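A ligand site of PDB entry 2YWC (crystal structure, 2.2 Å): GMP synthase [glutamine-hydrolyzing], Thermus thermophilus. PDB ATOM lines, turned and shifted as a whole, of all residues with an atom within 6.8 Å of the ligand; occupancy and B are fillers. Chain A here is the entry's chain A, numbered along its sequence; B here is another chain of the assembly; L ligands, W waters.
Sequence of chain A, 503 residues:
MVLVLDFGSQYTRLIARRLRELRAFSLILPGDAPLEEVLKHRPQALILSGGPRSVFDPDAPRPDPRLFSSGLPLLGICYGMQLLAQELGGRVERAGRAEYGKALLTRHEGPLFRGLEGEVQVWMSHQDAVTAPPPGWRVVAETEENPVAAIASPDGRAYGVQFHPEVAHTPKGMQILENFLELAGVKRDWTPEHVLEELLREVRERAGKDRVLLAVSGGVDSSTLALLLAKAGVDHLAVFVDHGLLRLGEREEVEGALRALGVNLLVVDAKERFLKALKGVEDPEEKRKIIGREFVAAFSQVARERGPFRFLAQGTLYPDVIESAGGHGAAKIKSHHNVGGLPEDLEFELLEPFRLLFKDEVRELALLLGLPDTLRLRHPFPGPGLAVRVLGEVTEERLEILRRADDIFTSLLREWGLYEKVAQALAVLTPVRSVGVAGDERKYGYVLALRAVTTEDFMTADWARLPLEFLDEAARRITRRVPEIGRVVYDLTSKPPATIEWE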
ATOM      1  N   ARG A 288      32.165 -18.212  33.468  1.00  0.00           N
ATOM      2  CA  ARG A 288      32.540 -16.979  32.786  1.00  0.00           C
ATOM      3  C   ARG A 288      33.739 -16.335  33.472  1.00  0.00           C
ATOM      4  O   ARG A 288      34.615 -15.783  32.809  1.00  0.00           O
ATOM      5  CB  ARG A 288      31.379 -15.992  32.756  1.00  0.00           C
ATOM      6  CG  ARG A 288      30.156 -16.442  31.960  1.00  0.00           C
ATOM      7  CD  ARG A 288      29.155 -15.291  31.893  1.00  0.00           C
ATOM      8  NE  ARG A 288      27.793 -15.695  31.526  1.00  0.00           N
ATOM      9  CZ  ARG A 288      27.423 -16.043  30.304  1.00  0.00           C
ATOM     10  NH1 ARG A 288      28.288 -16.046  29.314  1.00  0.00           N
ATOM     11  NH2 ARG A 288      26.157 -16.361  30.070  1.00  0.00           N
ATOM     12  N   PRO A 380      26.480 -14.079  15.774  1.00  0.00           N
ATOM     13  CA  PRO A 380      27.314 -13.814  16.942  1.00  0.00           C
ATOM     14  C   PRO A 380      27.522 -15.112  17.712  1.00  0.00           C
ATOM     15  O   PRO A 380      26.638 -15.973  17.732  1.00  0.00           O
ATOM     16  CB  PRO A 380      26.478 -12.833  17.764  1.00  0.00           C
ATOM     17  CG  PRO A 380      25.491 -12.262  16.759  1.00  0.00           C
ATOM     18  CD  PRO A 380      25.168 -13.429  15.902  1.00  0.00           C
ATOM     19  N   PHE A 381      28.684 -15.237  18.340  1.00  0.00           N
ATOM     20  CA  PHE A 381      29.023 -16.412  19.149  1.00  0.00           C
ATOM     21  C   PHE A 381      29.734 -15.833  20.367  1.00  0.00           C
ATOM     22  O   PHE A 381      30.628 -15.001  20.218  1.00  0.00           O
ATOM     23  CB  PHE A 381      29.949 -17.335  18.359  1.00  0.00           C
ATOM     24  CG  PHE A 381      30.170 -18.668  19.013  1.00  0.00           C
ATOM     25  CD1 PHE A 381      29.112 -19.573  19.114  1.00  0.00           C
ATOM     26  CD2 PHE A 381      31.412 -19.002  19.548  1.00  0.00           C
ATOM     27  CE1 PHE A 381      29.290 -20.805  19.747  1.00  0.00           C
ATOM     28  CE2 PHE A 381      31.598 -20.228  20.181  1.00  0.00           C
ATOM     29  CZ  PHE A 381      30.527 -21.131  20.279  1.00  0.00           C
ATOM     30  N   PRO A 382      29.368 -16.259  21.586  1.00  0.00           N
ATOM     31  CA  PRO A 382      29.987 -15.744  22.825  1.00  0.00           C
ATOM     32  C   PRO A 382      31.442 -16.107  23.146  1.00  0.00           C
ATOM     33  O   PRO A 382      31.924 -17.175  22.768  1.00  0.00           O
ATOM     34  CB  PRO A 382      29.032 -16.212  23.913  1.00  0.00           C
ATOM     35  CG  PRO A 382      28.541 -17.541  23.374  1.00  0.00           C
ATOM     36  CD  PRO A 382      28.356 -17.298  21.885  1.00  0.00           C
ATOM     37  N   GLY A 383      32.116 -15.196  23.852  1.00  0.00           N
ATOM     38  CA  GLY A 383      33.502 -15.416  24.242  1.00  0.00           C
ATOM     39  C   GLY A 383      33.682 -16.748  24.938  1.00  0.00           C
ATOM     40  O   GLY A 383      34.602 -17.488  24.613  1.00  0.00           O
ATOM     41  N   PRO A 384      32.835 -17.090  25.911  1.00  0.00           N
ATOM     42  CA  PRO A 384      32.954 -18.371  26.613  1.00  0.00           C
ATOM     43  C   PRO A 384      32.433 -19.555  25.783  1.00  0.00           C
ATOM     44  O   PRO A 384      32.363 -20.687  26.278  1.00  0.00           O
ATOM     45  CB  PRO A 384      32.142 -18.154  27.887  1.00  0.00           C
ATOM     46  CG  PRO A 384      31.124 -17.134  27.465  1.00  0.00           C
ATOM     47  CD  PRO A 384      31.936 -16.178  26.627  1.00  0.00           C
ATOM     48  N   GLY A 385      32.079 -19.282  24.528  1.00  0.00           N
ATOM     49  CA  GLY A 385      31.593 -20.310  23.621  1.00  0.00           C
ATOM     50  C   GLY A 385      30.665 -21.372  24.179  1.00  0.00           C
ATOM     51  O   GLY A 385      29.740 -21.085  24.935  1.00  0.00           O
ATOM     52  N   VAL A 388      28.964 -22.115  27.905  1.00  0.00           N
ATOM     53  CA  VAL A 388      27.701 -21.599  28.422  1.00  0.00           C
ATOM     54  C   VAL A 388      26.532 -22.268  27.718  1.00  0.00           C
ATOM     55  O   VAL A 388      25.390 -21.807  27.814  1.00  0.00           O
ATOM     56  CB  VAL A 388      27.582 -20.051  28.264  1.00  0.00           C
ATOM     57  CG1 VAL A 388      28.754 -19.365  28.945  1.00  0.00           C
ATOM     58  CG2 VAL A 388      27.492 -19.665  26.790  1.00  0.00           C
ATOM     59  N   ARG A 389      26.813 -23.363  27.010  1.00  0.00           N
ATOM     60  CA  ARG A 389      25.755 -24.086  26.303  1.00  0.00           C
ATOM     61  C   ARG A 389      25.599 -25.544  26.741  1.00  0.00           C
ATOM     62  O   ARG A 389      24.916 -26.343  26.083  1.00  0.00           O
ATOM     63  CB  ARG A 389      25.938 -23.934  24.801  1.00  0.00           C
ATOM     64  CG  ARG A 389      25.747 -22.469  24.379  1.00  0.00           C
ATOM     65  CD  ARG A 389      25.669 -22.259  22.882  1.00  0.00           C
ATOM     66  NE  ARG A 389      25.554 -20.847  22.554  1.00  0.00           N
ATOM     67  CZ  ARG A 389      25.799 -20.339  21.360  1.00  0.00           C
ATOM     68  NH1 ARG A 389      26.169 -21.146  20.372  1.00  0.00           N
ATOM     69  NH2 ARG A 389      25.698 -19.039  21.144  1.00  0.00           N
ATOM     70  N   GLN A 424      20.294 -15.103  15.520  1.00  0.00           N
ATOM     71  CA  GLN A 424      21.192 -16.025  16.207  1.00  0.00           C
ATOM     72  C   GLN A 424      20.516 -17.369  16.446  1.00  0.00           C
ATOM     73  O   GLN A 424      19.316 -17.430  16.679  1.00  0.00           O
ATOM     74  CB  GLN A 424      21.642 -15.421  17.542  1.00  0.00           C
ATOM     75  CG  GLN A 424      22.543 -16.320  18.384  1.00  0.00           C
ATOM     76  CD  GLN A 424      23.189 -15.586  19.562  1.00  0.00           C
ATOM     77  OE1 GLN A 424      22.559 -14.756  20.227  1.00  0.00           O
ATOM     78  NE2 GLN A 424      24.449 -15.906  19.836  1.00  0.00           N
ATOM     79  N   LEU A 426      21.315 -21.423  18.297  1.00  0.00           N
ATOM     80  CA  LEU A 426      22.225 -22.148  19.189  1.00  0.00           C
ATOM     81  C   LEU A 426      21.585 -23.415  19.736  1.00  0.00           C
ATOM     82  O   LEU A 426      20.360 -23.577  19.711  1.00  0.00           O
ATOM     83  CB  LEU A 426      22.665 -21.233  20.340  1.00  0.00           C
ATOM     84  CG  LEU A 426      21.578 -20.645  21.244  1.00  0.00           C
ATOM     85  CD1 LEU A 426      21.265 -21.627  22.352  1.00  0.00           C
ATOM     86  CD2 LEU A 426      22.053 -19.338  21.847  1.00  0.00           C
ATOM     87  N   PHE A 458      19.711  -6.937  20.522  1.00  0.00           N
ATOM     88  CA  PHE A 458      19.969  -8.120  21.344  1.00  0.00           C
ATOM     89  C   PHE A 458      19.646  -8.050  22.848  1.00  0.00           C
ATOM     90  O   PHE A 458      20.259  -8.752  23.648  1.00  0.00           O
ATOM     91  CB  PHE A 458      21.423  -8.557  21.143  1.00  0.00           C
ATOM     92  CG  PHE A 458      21.632  -9.354  19.890  1.00  0.00           C
ATOM     93  CD1 PHE A 458      22.176  -8.758  18.754  1.00  0.00           C
ATOM     94  CD2 PHE A 458      21.213 -10.685  19.823  1.00  0.00           C
ATOM     95  CE1 PHE A 458      22.298  -9.474  17.568  1.00  0.00           C
ATOM     96  CE2 PHE A 458      21.327 -11.407  18.635  1.00  0.00           C
ATOM     97  CZ  PHE A 458      21.879 -10.805  17.500  1.00  0.00           C
ATOM     98  N   MET A 459      18.593  -7.241  22.956  1.00  0.00           N
ATOM     99  CA  MET A 459      18.303  -6.673  24.268  1.00  0.00           C
ATOM    100  C   MET A 459      16.819  -6.850  24.580  1.00  0.00           C
ATOM    101  O   MET A 459      16.425  -7.045  25.733  1.00  0.00           O
ATOM    102  CB  MET A 459      18.715  -5.200  24.293  1.00  0.00           C
ATOM    103  CG  MET A 459      20.083  -4.954  24.927  1.00  0.00           C
ATOM    104  SD  MET A 459      20.738  -3.289  24.647  1.00  0.00           S
ATOM    105  CE  MET A 459      19.379  -2.263  25.294  1.00  0.00           C
ATOM    106  N   LYS A 495      12.560 -12.649  24.848  1.00  0.00           N
ATOM    107  CA  LYS A 495      13.300 -11.799  25.774  1.00  0.00           C
ATOM    108  C   LYS A 495      12.776 -10.366  25.706  1.00  0.00           C
ATOM    109  O   LYS A 495      12.931  -9.701  24.688  1.00  0.00           O
ATOM    110  CB  LYS A 495      14.794 -11.791  25.426  1.00  0.00           C
ATOM    111  CG  LYS A 495      15.603 -10.839  26.305  1.00  0.00           C
ATOM    112  CD  LYS A 495      17.064 -10.791  25.888  1.00  0.00           C
ATOM    113  CE  LYS A 495      17.924 -10.161  26.985  1.00  0.00           C
ATOM    114  NZ  LYS A 495      19.369 -10.191  26.654  1.00  0.00           N
ATOM    115  N   ALA A 498      13.113 -14.016  29.124  1.00  0.00           N
ATOM    116  CA  ALA A 498      14.309 -14.834  29.212  1.00  0.00           C
ATOM    117  C   ALA A 498      15.475 -14.371  28.347  1.00  0.00           C
ATOM    118  O   ALA A 498      15.298 -13.704  27.339  1.00  0.00           O
ATOM    119  CB  ALA A 498      13.969 -16.290  28.875  1.00  0.00           C
ATOM    120  N   THR A 499      16.667 -14.756  28.764  1.00  0.00           N
ATOM    121  CA  THR A 499      17.879 -14.421  28.044  1.00  0.00           C
ATOM    122  C   THR A 499      17.978 -15.248  26.769  1.00  0.00           C
ATOM    123  O   THR A 499      17.275 -16.238  26.600  1.00  0.00           O
ATOM    124  CB  THR A 499      19.102 -14.712  28.923  1.00  0.00           C
ATOM    125  OG1 THR A 499      18.946 -16.000  29.514  1.00  0.00           O
ATOM    126  CG2 THR A 499      19.253 -13.648  30.001  1.00  0.00           C
ATOM    127  N   ILE A 500      18.873 -14.847  25.870  1.00  0.00           N
ATOM    128  CA  ILE A 500      19.047 -15.597  24.640  1.00  0.00           C
ATOM    129  C   ILE A 500      19.770 -16.917  24.967  1.00  0.00           C
ATOM    130  O   ILE A 500      19.304 -17.986  24.579  1.00  0.00           O
ATOM    131  CB  ILE A 500      19.835 -14.768  23.602  1.00  0.00           C
ATOM    132  CG1 ILE A 500      18.978 -13.573  23.172  1.00  0.00           C
ATOM    133  CG2 ILE A 500      20.185 -15.635  22.389  1.00  0.00           C
ATOM    134  CD1 ILE A 500      19.567 -12.594  22.114  1.00  0.00           C
ATOM    135  N   GLU A 501      20.887 -16.834  25.697  1.00  0.00           N
ATOM    136  CA  GLU A 501      21.623 -18.027  26.106  1.00  0.00           C
ATOM    137  C   GLU A 501      20.871 -18.645  27.278  1.00  0.00           C
ATOM    138  O   GLU A 501      20.092 -17.971  27.948  1.00  0.00           O
ATOM    139  CB  GLU A 501      23.043 -17.670  26.582  1.00  0.00           C
ATOM    140  CG  GLU A 501      23.961 -17.032  25.543  1.00  0.00           C
ATOM    141  CD  GLU A 501      24.334 -17.960  24.392  1.00  0.00           C
ATOM    142  OE1 GLU A 501      24.348 -19.201  24.584  1.00  0.00           O
ATOM    143  OE2 GLU A 501      24.641 -17.435  23.305  1.00  0.00           O
ATOM    144  N   TRP A 502      21.096 -19.938  27.535  1.00  0.00           N
ATOM    145  CA  TRP A 502      20.416 -20.612  28.632  1.00  0.00           C
ATOM    146  C   TRP A 502      21.128 -20.426  29.964  1.00  0.00           C
ATOM    147  O   TRP A 502      20.641 -20.860  31.006  1.00  0.00           O
ATOM    148  CB  TRP A 502      20.259 -22.092  28.315  1.00  0.00           C
ATOM    149  CG  TRP A 502      19.012 -22.422  27.551  1.00  0.00           C
ATOM    150  CD1 TRP A 502      18.462 -21.688  26.528  1.00  0.00           C
ATOM    151  CD2 TRP A 502      18.155 -23.548  27.750  1.00  0.00           C
ATOM    152  NE1 TRP A 502      17.309 -22.297  26.089  1.00  0.00           N
ATOM    153  CE2 TRP A 502      17.096 -23.434  26.813  1.00  0.00           C
ATOM    154  CE3 TRP A 502      18.168 -24.632  28.625  1.00  0.00           C
ATOM    155  CZ2 TRP A 502      16.060 -24.379  26.738  1.00  0.00           C
ATOM    156  CZ3 TRP A 502      17.132 -25.577  28.551  1.00  0.00           C
ATOM    157  CH2 TRP A 502      16.101 -25.449  27.607  1.00  0.00           C
ATOM    158  N   GLU A 503      22.289 -19.789  29.936  1.00  0.00           N
ATOM    159  CA  GLU A 503      23.017 -19.540  31.175  1.00  0.00           C
ATOM    160  C   GLU A 503      24.073 -18.473  30.976  1.00  0.00           C
ATOM    161  O   GLU A 503      24.275 -18.068  29.814  1.00  0.00           O
ATOM    162  CB  GLU A 503      23.675 -20.831  31.690  1.00  0.00           C
ATOM    163  CG  GLU A 503      24.827 -21.349  30.860  1.00  0.00           C
ATOM    164  CD  GLU A 503      25.545 -22.521  31.523  1.00  0.00           C
ATOM    165  OE1 GLU A 503      24.879 -23.533  31.831  1.00  0.00           O
ATOM    166  OE2 GLU A 503      26.764 -22.431  31.731  1.00  0.00           O
ATOM    167  OXT GLU A 503      24.673 -18.055  31.988  1.00  0.00           O
ATOM    168  N   ARG B 487      11.512 -20.561  31.681  1.00  0.00           N
ATOM    169  CA  ARG B 487      11.625 -20.927  30.281  1.00  0.00           C
ATOM    170  C   ARG B 487      10.672 -22.070  29.901  1.00  0.00           C
ATOM    171  O   ARG B 487      10.542 -23.063  30.636  1.00  0.00           O
ATOM    172  CB  ARG B 487      13.075 -21.326  29.987  1.00  0.00           C
ATOM    173  CG  ARG B 487      13.455 -21.308  28.521  1.00  0.00           C
ATOM    174  CD  ARG B 487      14.924 -21.592  28.334  1.00  0.00           C
ATOM    175  NE  ARG B 487      15.814 -20.540  28.844  1.00  0.00           N
ATOM    176  CZ  ARG B 487      16.166 -19.438  28.185  1.00  0.00           C
ATOM    177  NH1 ARG B 487      15.726 -19.202  26.948  1.00  0.00           N
ATOM    178  NH2 ARG B 487      17.007 -18.571  28.753  1.00  0.00           N
HETATM  179  P1  LIG L   1      21.713 -13.022  26.755  1.00  0.00           P
HETATM  180  O1  LIG L   1      22.341 -11.979  27.822  1.00  0.00           O
HETATM  181  O2  LIG L   1      21.712 -14.507  27.385  1.00  0.00           O
HETATM  182  O3  LIG L   1      22.605 -13.065  25.443  1.00  0.00           O
HETATM  183  O4  LIG L   1      20.325 -12.616  26.431  1.00  0.00           O
HETATM  184  C1  LIG L   1      22.536 -11.808  24.759  1.00  0.00           C
HETATM  185  C2  LIG L   1      23.599 -11.798  23.659  1.00  0.00           C
HETATM  186  O5  LIG L   1      24.931 -11.688  24.259  1.00  0.00           O
HETATM  187  C3  LIG L   1      25.648 -12.929  24.041  1.00  0.00           C
HETATM  188  N1  LIG L   1      26.336 -13.349  25.264  1.00  0.00           N
HETATM  189  C4  LIG L   1      27.668 -13.227  25.462  1.00  0.00           C
HETATM  190  N2  LIG L   1      28.718 -12.749  24.670  1.00  0.00           N
HETATM  191  N3  LIG L   1      30.297 -13.213  26.371  1.00  0.00           N
HETATM  192  C5  LIG L   1      30.003 -12.745  25.133  1.00  0.00           C
HETATM  193  O6  LIG L   1      30.900 -12.323  24.419  1.00  0.00           O
HETATM  194  C6  LIG L   1      29.323 -13.701  27.206  1.00  0.00           C
HETATM  195  O7  LIG L   1      29.600 -14.105  28.310  1.00  0.00           O
HETATM  196  C7  LIG L   1      27.917 -13.723  26.736  1.00  0.00           C
HETATM  197  N4  LIG L   1      26.728 -14.116  27.264  1.00  0.00           N
HETATM  198  C8  LIG L   1      25.786 -13.900  26.399  1.00  0.00           C
HETATM  199  C9  LIG L   1      24.629 -13.974  23.539  1.00  0.00           C
HETATM  200  O8  LIG L   1      25.240 -14.964  22.714  1.00  0.00           O
HETATM  201  C10 LIG L   1      23.590 -13.106  22.816  1.00  0.00           C
HETATM  202  O9  LIG L   1      24.007 -12.838  21.454  1.00  0.00           O
HETATM  203  O   HOH W   1      22.994 -15.399  29.586  1.00  0.00           O
HETATM  204  O   HOH W   2      21.075 -10.784  29.785  1.00  0.00           O
HETATM  205  O   HOH W   3      31.880 -13.633  29.877  1.00  0.00           O
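Merely in contact with the ligand: Pro 382 (3.6 Å), Pro 384 (3.4 Å), Phe 458 (3.9 Å) and Thr 499 (3.0 Å).
Hydrophobic or aromatic side chains within 4 Å of the ligand: Pro 382, Pro 384, Phe 458 and Ile 500.
Of the 21 residues printed, 10 come within 4 Å of the ligand.
Along chain A the residues within 4 Å of the ligand span positions 288 to 501.
The nearest printed residue that does not touch the ligand is Arg 389 (4.4 Å).
NH2 of Arg 288 lies within salt-bridge range of O of Glu 503 (2.6 Å).
NE2 of Gln 424 lies within hydrogen-bond range of O of Pro 380, 3.0 Å away.
The backbone carbonyl oxygen of Glu 501 is in hydrogen-bond range of the guanidinium group of Arg 487 of chain B.
The backbone carbonyl oxygen of Phe 458 sits at hydrogen-bond distance from the side-chain amino group of Lys 495 (3.4 Å).
The side-chain carboxylate (OE1) of Glu 501 is in salt-bridge range of the guanidinium group (NE) of Arg 389 (2.9 Å).
The backbone carbonyl oxygen (O) of Glu 501 sits at hydrogen-bond distance from the side-chain hydroxyl (OG1) of Thr 499, 2.8 Å away.
O of Thr 499 sits at hydrogen-bond distance from NH2 of Arg 487 of chain B.
O6 of the ligand lies within hydrogen-bond range of N of Gly 383 (3.2 Å).
The side-chain amino group (NZ) of Lys 495 lies within salt-bridge range of an oxygen (O4) of the ligand, 2.6 Å away.
NH1 of Arg 288 sits at hydrogen-bond distance from O7 of the ligand (2.5 Å).
The backbone NH (N) of Glu 501 lies within hydrogen-bond range of an oxygen (O2) of the ligand.
The side-chain carboxylate (OE2) of Glu 501 is in hydrogen-bond range of an oxygen (O8) of the ligand (2.6 Å).
The backbone NH (N) of Ile 500 sits at hydrogen-bond distance from an oxygen (O4) of the ligand, at 2.7 Å.
The side-chain amide oxygen of Gln 424 lies within hydrogen-bond range of an oxygen (O9) of the ligand.
Water W1 lies within hydrogen-bond range of O2 of the ligand (2.7 Å), O of Glu 503 (3.0 Å) and NH2 of Arg 288 (3.3 Å).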
